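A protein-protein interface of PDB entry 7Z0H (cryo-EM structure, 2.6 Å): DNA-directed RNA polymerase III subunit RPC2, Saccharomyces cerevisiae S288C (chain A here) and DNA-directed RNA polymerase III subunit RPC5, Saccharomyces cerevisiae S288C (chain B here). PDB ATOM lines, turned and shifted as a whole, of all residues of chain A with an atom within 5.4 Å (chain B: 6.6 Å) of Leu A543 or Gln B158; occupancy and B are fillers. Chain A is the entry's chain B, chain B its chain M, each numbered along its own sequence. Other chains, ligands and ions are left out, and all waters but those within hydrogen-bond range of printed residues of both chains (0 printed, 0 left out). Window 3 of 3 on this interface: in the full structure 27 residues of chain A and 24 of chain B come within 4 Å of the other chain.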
ATOM      1  N   GLU A 539      13.884   6.107 -14.221  1.00  0.00           N
ATOM      2  CA  GLU A 539      15.299   5.939 -13.936  1.00  0.00           C
ATOM      3  C   GLU A 539      15.517   4.638 -13.181  1.00  0.00           C
ATOM      4  O   GLU A 539      14.891   4.407 -12.144  1.00  0.00           O
ATOM      5  CB  GLU A 539      15.820   7.115 -13.115  1.00  0.00           C
ATOM      6  CG  GLU A 539      15.116   8.411 -13.421  1.00  0.00           C
ATOM      7  CD  GLU A 539      16.045   9.589 -13.322  1.00  0.00           C
ATOM      8  OE1 GLU A 539      17.194   9.395 -12.877  1.00  0.00           O
ATOM      9  OE2 GLU A 539      15.639  10.700 -13.708  1.00  0.00           O
ATOM     10  N   ASP A 540      16.411   3.800 -13.698  1.00  0.00           N
ATOM     11  CA  ASP A 540      16.683   2.519 -13.065  1.00  0.00           C
ATOM     12  C   ASP A 540      17.174   2.717 -11.637  1.00  0.00           C
ATOM     13  O   ASP A 540      17.853   3.697 -11.319  1.00  0.00           O
ATOM     14  CB  ASP A 540      17.721   1.738 -13.870  1.00  0.00           C
ATOM     15  CG  ASP A 540      17.556   0.238 -13.738  1.00  0.00           C
ATOM     16  OD1 ASP A 540      17.243  -0.235 -12.624  1.00  0.00           O
ATOM     17  OD2 ASP A 540      17.743  -0.471 -14.749  1.00  0.00           O
ATOM     18  N   ILE A 541      16.813   1.770 -10.769  1.00  0.00           N
ATOM     19  CA  ILE A 541      17.207   1.834  -9.368  1.00  0.00           C
ATOM     20  C   ILE A 541      18.718   1.819  -9.213  1.00  0.00           C
ATOM     21  O   ILE A 541      19.234   2.166  -8.145  1.00  0.00           O
ATOM     22  CB  ILE A 541      16.557   0.676  -8.585  1.00  0.00           C
ATOM     23  CG1 ILE A 541      16.894  -0.664  -9.238  1.00  0.00           C
ATOM     24  CG2 ILE A 541      15.056   0.872  -8.499  1.00  0.00           C
ATOM     25  CD1 ILE A 541      16.499  -1.862  -8.408  1.00  0.00           C
ATOM     26  N   THR A 542      19.448   1.431 -10.259  1.00  0.00           N
ATOM     27  CA  THR A 542      20.902   1.500 -10.222  1.00  0.00           C
ATOM     28  C   THR A 542      21.434   2.908 -10.482  1.00  0.00           C
ATOM     29  O   THR A 542      22.631   3.144 -10.295  1.00  0.00           O
ATOM     30  CB  THR A 542      21.497   0.511 -11.226  1.00  0.00           C
ATOM     31  OG1 THR A 542      21.132   0.896 -12.556  1.00  0.00           O
ATOM     32  CG2 THR A 542      20.992  -0.899 -10.956  1.00  0.00           C
ATOM     33  N   LEU A 543      20.585   3.846 -10.908  1.00  0.00           N
ATOM     34  CA  LEU A 543      20.958   5.254 -11.020  1.00  0.00           C
ATOM     35  C   LEU A 543      20.441   6.110  -9.875  1.00  0.00           C
ATOM     36  O   LEU A 543      20.726   7.311  -9.842  1.00  0.00           O
ATOM     37  CB  LEU A 543      20.445   5.862 -12.330  1.00  0.00           C
ATOM     38  CG  LEU A 543      21.172   5.619 -13.644  1.00  0.00           C
ATOM     39  CD1 LEU A 543      22.666   5.867 -13.466  1.00  0.00           C
ATOM     40  CD2 LEU A 543      20.891   4.226 -14.116  1.00  0.00           C
ATOM     41  N   ILE A 544      19.681   5.540  -8.951  1.00  0.00           N
ATOM     42  CA  ILE A 544      19.034   6.308  -7.899  1.00  0.00           C
ATOM     43  C   ILE A 544      19.810   6.111  -6.608  1.00  0.00           C
ATOM     44  O   ILE A 544      20.351   5.027  -6.354  1.00  0.00           O
ATOM     45  CB  ILE A 544      17.558   5.903  -7.723  1.00  0.00           C
ATOM     46  CG1 ILE A 544      16.871   5.777  -9.082  1.00  0.00           C
ATOM     47  CG2 ILE A 544      16.825   6.922  -6.866  1.00  0.00           C
ATOM     48  CD1 ILE A 544      15.525   5.103  -9.014  1.00  0.00           C
ATOM     49  N   ASP A 545      19.877   7.162  -5.804  1.00  0.00           N
ATOM     50  CA  ASP A 545      20.420   7.058  -4.462  1.00  0.00           C
ATOM     51  C   ASP A 545      19.300   6.791  -3.464  1.00  0.00           C
ATOM     52  O   ASP A 545      18.129   7.086  -3.708  1.00  0.00           O
ATOM     53  CB  ASP A 545      21.183   8.327  -4.081  1.00  0.00           C
ATOM     54  CG  ASP A 545      20.279   9.537  -3.950  1.00  0.00           C
ATOM     55  OD1 ASP A 545      19.218   9.564  -4.608  1.00  0.00           O
ATOM     56  OD2 ASP A 545      20.627  10.456  -3.181  1.00  0.00           O
ATOM     57  N   VAL B  87      30.724   6.772 -14.634  1.00  0.00           N
ATOM     58  CA  VAL B  87      30.214   7.772 -13.702  1.00  0.00           C
ATOM     59  C   VAL B  87      30.278   7.196 -12.296  1.00  0.00           C
ATOM     60  O   VAL B  87      29.771   6.096 -12.046  1.00  0.00           O
ATOM     61  CB  VAL B  87      28.780   8.207 -14.058  1.00  0.00           C
ATOM     62  CG1 VAL B  87      28.103   8.842 -12.857  1.00  0.00           C
ATOM     63  CG2 VAL B  87      28.812   9.185 -15.212  1.00  0.00           C
ATOM     64  N   GLN B  89      29.260   7.289  -8.432  1.00  0.00           N
ATOM     65  CA  GLN B  89      28.206   7.726  -7.523  1.00  0.00           C
ATOM     66  C   GLN B  89      28.684   7.487  -6.094  1.00  0.00           C
ATOM     67  O   GLN B  89      28.562   6.378  -5.567  1.00  0.00           O
ATOM     68  CB  GLN B  89      26.901   6.985  -7.806  1.00  0.00           C
ATOM     69  CG  GLN B  89      26.381   7.128  -9.225  1.00  0.00           C
ATOM     70  CD  GLN B  89      24.881   7.356  -9.273  1.00  0.00           C
ATOM     71  OE1 GLN B  89      24.395   8.219 -10.001  1.00  0.00           O
ATOM     72  NE2 GLN B  89      24.141   6.586  -8.485  1.00  0.00           N
ATOM     73  N   VAL B 153      27.456  -0.743 -13.094  1.00  0.00           N
ATOM     74  CA  VAL B 153      26.303  -1.447 -13.641  1.00  0.00           C
ATOM     75  C   VAL B 153      26.025  -0.918 -15.039  1.00  0.00           C
ATOM     76  O   VAL B 153      25.914   0.297 -15.244  1.00  0.00           O
ATOM     77  CB  VAL B 153      25.069  -1.304 -12.733  1.00  0.00           C
ATOM     78  CG1 VAL B 153      25.168  -2.260 -11.554  1.00  0.00           C
ATOM     79  CG2 VAL B 153      24.934   0.124 -12.241  1.00  0.00           C
ATOM     80  N   ASN B 155      24.086   0.307 -17.731  1.00  0.00           N
ATOM     81  CA  ASN B 155      22.785   0.894 -18.008  1.00  0.00           C
ATOM     82  C   ASN B 155      22.878   1.770 -19.246  1.00  0.00           C
ATOM     83  O   ASN B 155      23.814   2.565 -19.391  1.00  0.00           O
ATOM     84  CB  ASN B 155      22.269   1.655 -16.788  1.00  0.00           C
ATOM     85  CG  ASN B 155      20.897   1.180 -16.370  1.00  0.00           C
ATOM     86  OD1 ASN B 155      20.162   0.610 -17.177  1.00  0.00           O
ATOM     87  ND2 ASN B 155      20.598   1.286 -15.084  1.00  0.00           N
ATOM     88  N   ASN B 156      21.924   1.587 -20.149  1.00  0.00           N
ATOM     89  CA  ASN B 156      21.930   2.204 -21.463  1.00  0.00           C
ATOM     90  C   ASN B 156      21.085   3.470 -21.464  1.00  0.00           C
ATOM     91  O   ASN B 156      20.276   3.709 -20.565  1.00  0.00           O
ATOM     92  CB  ASN B 156      21.412   1.221 -22.515  1.00  0.00           C
ATOM     93  CG  ASN B 156      22.315   0.015 -22.680  1.00  0.00           C
ATOM     94  OD1 ASN B 156      21.854  -1.126 -22.687  1.00  0.00           O
ATOM     95  ND2 ASN B 156      23.614   0.263 -22.801  1.00  0.00           N
ATOM     96  N   GLY B 157      21.290   4.287 -22.493  1.00  0.00           N
ATOM     97  CA  GLY B 157      20.574   5.533 -22.631  1.00  0.00           C
ATOM     98  C   GLY B 157      21.136   6.690 -21.837  1.00  0.00           C
ATOM     99  O   GLY B 157      20.548   7.778 -21.862  1.00  0.00           O
ATOM    100  N   GLN B 158      22.253   6.500 -21.142  1.00  0.00           N
ATOM    101  CA  GLN B 158      22.857   7.546 -20.327  1.00  0.00           C
ATOM    102  C   GLN B 158      24.002   8.199 -21.090  1.00  0.00           C
ATOM    103  O   GLN B 158      24.890   7.507 -21.599  1.00  0.00           O
ATOM    104  CB  GLN B 158      23.358   6.979 -18.998  1.00  0.00           C
ATOM    105  CG  GLN B 158      22.698   5.673 -18.599  1.00  0.00           C
ATOM    106  CD  GLN B 158      21.304   5.875 -18.038  1.00  0.00           C
ATOM    107  OE1 GLN B 158      21.129   6.505 -16.997  1.00  0.00           O
ATOM    108  NE2 GLN B 158      20.304   5.344 -18.731  1.00  0.00           N
ATOM    109  N   TYR B 159      23.975   9.528 -21.168  1.00  0.00           N
ATOM    110  CA  TYR B 159      25.004  10.301 -21.856  1.00  0.00           C
ATOM    111  C   TYR B 159      25.421  11.461 -20.963  1.00  0.00           C
ATOM    112  O   TYR B 159      24.619  12.362 -20.699  1.00  0.00           O
ATOM    113  CB  TYR B 159      24.505  10.825 -23.204  1.00  0.00           C
ATOM    114  CG  TYR B 159      24.012   9.772 -24.170  1.00  0.00           C
ATOM    115  CD1 TYR B 159      22.713   9.288 -24.098  1.00  0.00           C
ATOM    116  CD2 TYR B 159      24.839   9.279 -25.168  1.00  0.00           C
ATOM    117  CE1 TYR B 159      22.259   8.332 -24.985  1.00  0.00           C
ATOM    118  CE2 TYR B 159      24.394   8.323 -26.058  1.00  0.00           C
ATOM    119  CZ  TYR B 159      23.103   7.853 -25.962  1.00  0.00           C
ATOM    120  OH  TYR B 159      22.655   6.902 -26.849  1.00  0.00           O
ATOM    121  N   ALA B 160      26.669  11.446 -20.504  1.00  0.00           N
ATOM    122  CA  ALA B 160      27.222  12.618 -19.841  1.00  0.00           C
ATOM    123  C   ALA B 160      27.497  13.705 -20.871  1.00  0.00           C
ATOM    124  O   ALA B 160      27.985  13.430 -21.970  1.00  0.00           O
ATOM    125  CB  ALA B 160      28.502  12.259 -19.089  1.00  0.00           C
ATOM    126  N   VAL B 171      28.266  12.460 -24.598  1.00  0.00           N
ATOM    127  CA  VAL B 171      29.220  11.361 -24.572  1.00  0.00           C
ATOM    128  C   VAL B 171      28.548  10.183 -23.874  1.00  0.00           C
ATOM    129  O   VAL B 171      28.106  10.319 -22.731  1.00  0.00           O
ATOM    130  CB  VAL B 171      30.527  11.740 -23.855  1.00  0.00           C
ATOM    131  CG1 VAL B 171      31.529  10.598 -23.939  1.00  0.00           C
ATOM    132  CG2 VAL B 171      31.108  13.014 -24.445  1.00  0.00           C
ATOM    133  N   PRO B 172      28.444   9.018 -24.512  1.00  0.00           N
ATOM    134  CA  PRO B 172      27.742   7.891 -23.885  1.00  0.00           C
ATOM    135  C   PRO B 172      28.436   7.435 -22.610  1.00  0.00           C
ATOM    136  O   PRO B 172      29.665   7.459 -22.504  1.00  0.00           O
ATOM    137  CB  PRO B 172      27.774   6.807 -24.968  1.00  0.00           C
ATOM    138  CG  PRO B 172      28.951   7.156 -25.812  1.00  0.00           C
ATOM    139  CD  PRO B 172      29.006   8.654 -25.823  1.00  0.00           C
ATOM    140  N   ILE B 173      27.632   7.014 -21.642  1.00  0.00           N
ATOM    141  CA  ILE B 173      28.140   6.577 -20.349  1.00  0.00           C
ATOM    142  C   ILE B 173      28.334   5.067 -20.369  1.00  0.00           C
ATOM    143  O   ILE B 173      27.539   4.322 -20.951  1.00  0.00           O
ATOM    144  CB  ILE B 173      27.178   7.010 -19.225  1.00  0.00           C
ATOM    145  CG1 ILE B 173      27.257   8.519 -19.012  1.00  0.00           C
ATOM    146  CG2 ILE B 173      27.509   6.298 -17.929  1.00  0.00           C
ATOM    147  CD1 ILE B 173      26.444   8.996 -17.841  1.00  0.00           C
ATOM    148  N   GLU B 174      29.410   4.608 -19.735  1.00  0.00           N
ATOM    149  CA  GLU B 174      29.701   3.188 -19.601  1.00  0.00           C
ATOM    150  C   GLU B 174      29.683   2.818 -18.125  1.00  0.00           C
ATOM    151  O   GLU B 174      30.516   3.305 -17.354  1.00  0.00           O
ATOM    152  CB  GLU B 174      31.056   2.846 -20.223  1.00  0.00           C
ATOM    153  CG  GLU B 174      30.975   1.962 -21.453  1.00  0.00           C
ATOM    154  CD  GLU B 174      30.509   0.557 -21.130  1.00  0.00           C
ATOM    155  OE1 GLU B 174      30.882   0.039 -20.057  1.00  0.00           O
ATOM    156  OE2 GLU B 174      29.769  -0.029 -21.949  1.00  0.00           O
ATOM    157  N   VAL B 176      27.743   3.039 -15.037  1.00  0.00           N
ATOM    158  CA  VAL B 176      27.643   3.863 -13.836  1.00  0.00           C
ATOM    159  C   VAL B 176      27.951   3.019 -12.607  1.00  0.00           C
ATOM    160  O   VAL B 176      27.548   1.853 -12.512  1.00  0.00           O
ATOM    161  CB  VAL B 176      26.244   4.493 -13.734  1.00  0.00           C
ATOM    162  CG1 VAL B 176      26.241   5.626 -12.723  1.00  0.00           C
ATOM    163  CG2 VAL B 176      25.781   4.980 -15.094  1.00  0.00           C
ATOM    164  N   GLN B 178      28.076   2.763  -8.304  1.00  0.00           N
ATOM    165  CA  GLN B 178      27.541   3.238  -7.030  1.00  0.00           C
ATOM    166  C   GLN B 178      28.517   2.825  -5.931  1.00  0.00           C
ATOM    167  O   GLN B 178      28.513   1.676  -5.482  1.00  0.00           O
ATOM    168  CB  GLN B 178      26.144   2.677  -6.784  1.00  0.00           C
ATOM    169  CG  GLN B 178      25.043   3.450  -7.490  1.00  0.00           C
ATOM    170  CD  GLN B 178      23.816   3.640  -6.626  1.00  0.00           C
ATOM    171  OE1 GLN B 178      23.133   4.659  -6.714  1.00  0.00           O
ATOM    172  NE2 GLN B 178      23.523   2.652  -5.787  1.00  0.00           N
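The side-chain amide nitrogen (ND2) of Asn B155 lies close to the side-chain carboxylate (OD2) of Asp A540, 3.4 Å away.
ND2 of Asn B155 sits at hydrogen-bond distance from OG1 of Thr A542 (2.6 Å).
The side-chain amide oxygen (OE1) of Gln B178 lies close to the backbone carbonyl oxygen (O) of Ile A544, at 2.8 Å.
The side-chain amide nitrogen (NE2) of Gln B89 sits at hydrogen-bond distance from the side-chain amide oxygen (OE1) of Gln B178, 2.8 Å away.
N of Val B153 lies within hydrogen-bond range of O of Val B176 (2.7 Å).
The side-chain amide nitrogen (NE2) of Gln B158 lies within hydrogen-bond range of the backbone carbonyl oxygen (O) of Asn B156 (2.5 Å).
O of Gln B158 sits at hydrogen-bond distance from N of Ile B173, at 2.8 Å.
Val B153 touches Thr A542 (CG2 to CB, 3.6 Å).
CG of Gln B178 touches O of Thr A542 (3.7 Å).
O of Leu A543 touches NE2 of Gln B89 (3.7 Å).
ND2 of Asn B155 touches CD2 of Leu A543, 3.1 Å away.
Leu A543 touches Gln B158 (CG to OE1, 3.5 Å).
CG2 of Val B176 touches CD1 of Leu A543, at 3.6 Å.
Of chain B, only Gln B89, Asn B155, Gln B158 and Val B176 come within 4 Å of Leu A543.
Of chain A, only Leu A543 comes within 4 Å of Gln B158.
Of the printed residues of chain B, Asp A540 touches Asn B155.
Of the printed residues of chain B, Ile A544 touches Gln B178.
Printed residues of chain A within 4 Å of Val B153: Thr A542.
Of the printed residues of chain A, Gln B178 touches Thr A542 and Ile A544.
The nearest residue of chain B that does not touch Leu A543 is Gln B178 (4.4 Å).
The nearest printed residue of chain B that does not touch Thr A542 is Gln B89 (4.2 Å).
Printed residues of chain A that touch a printed residue of chain B: Asp A540, Thr A542, Leu A543 and Ile A544.
Hydrophobic or aromatic side chains of chain A within 4 Å of the printed part of chain B: Leu A543.
Of the 15 printed residues of chain B, 6 touch a printed residue of chain A.
Printed residues of chain B that touch a printed residue of chain A: Gln B89, Val B153, Asn B155, Gln B158, Val B176 and Gln B178.
Hydrophobic or aromatic side chains of chain B that line the printed part of chain A: Val B153 and Val B176.
Among the printed residues, no Asp or Glu carboxylate lies within 4 Å of a Lys or Arg side-chain nitrogen of the other chain.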
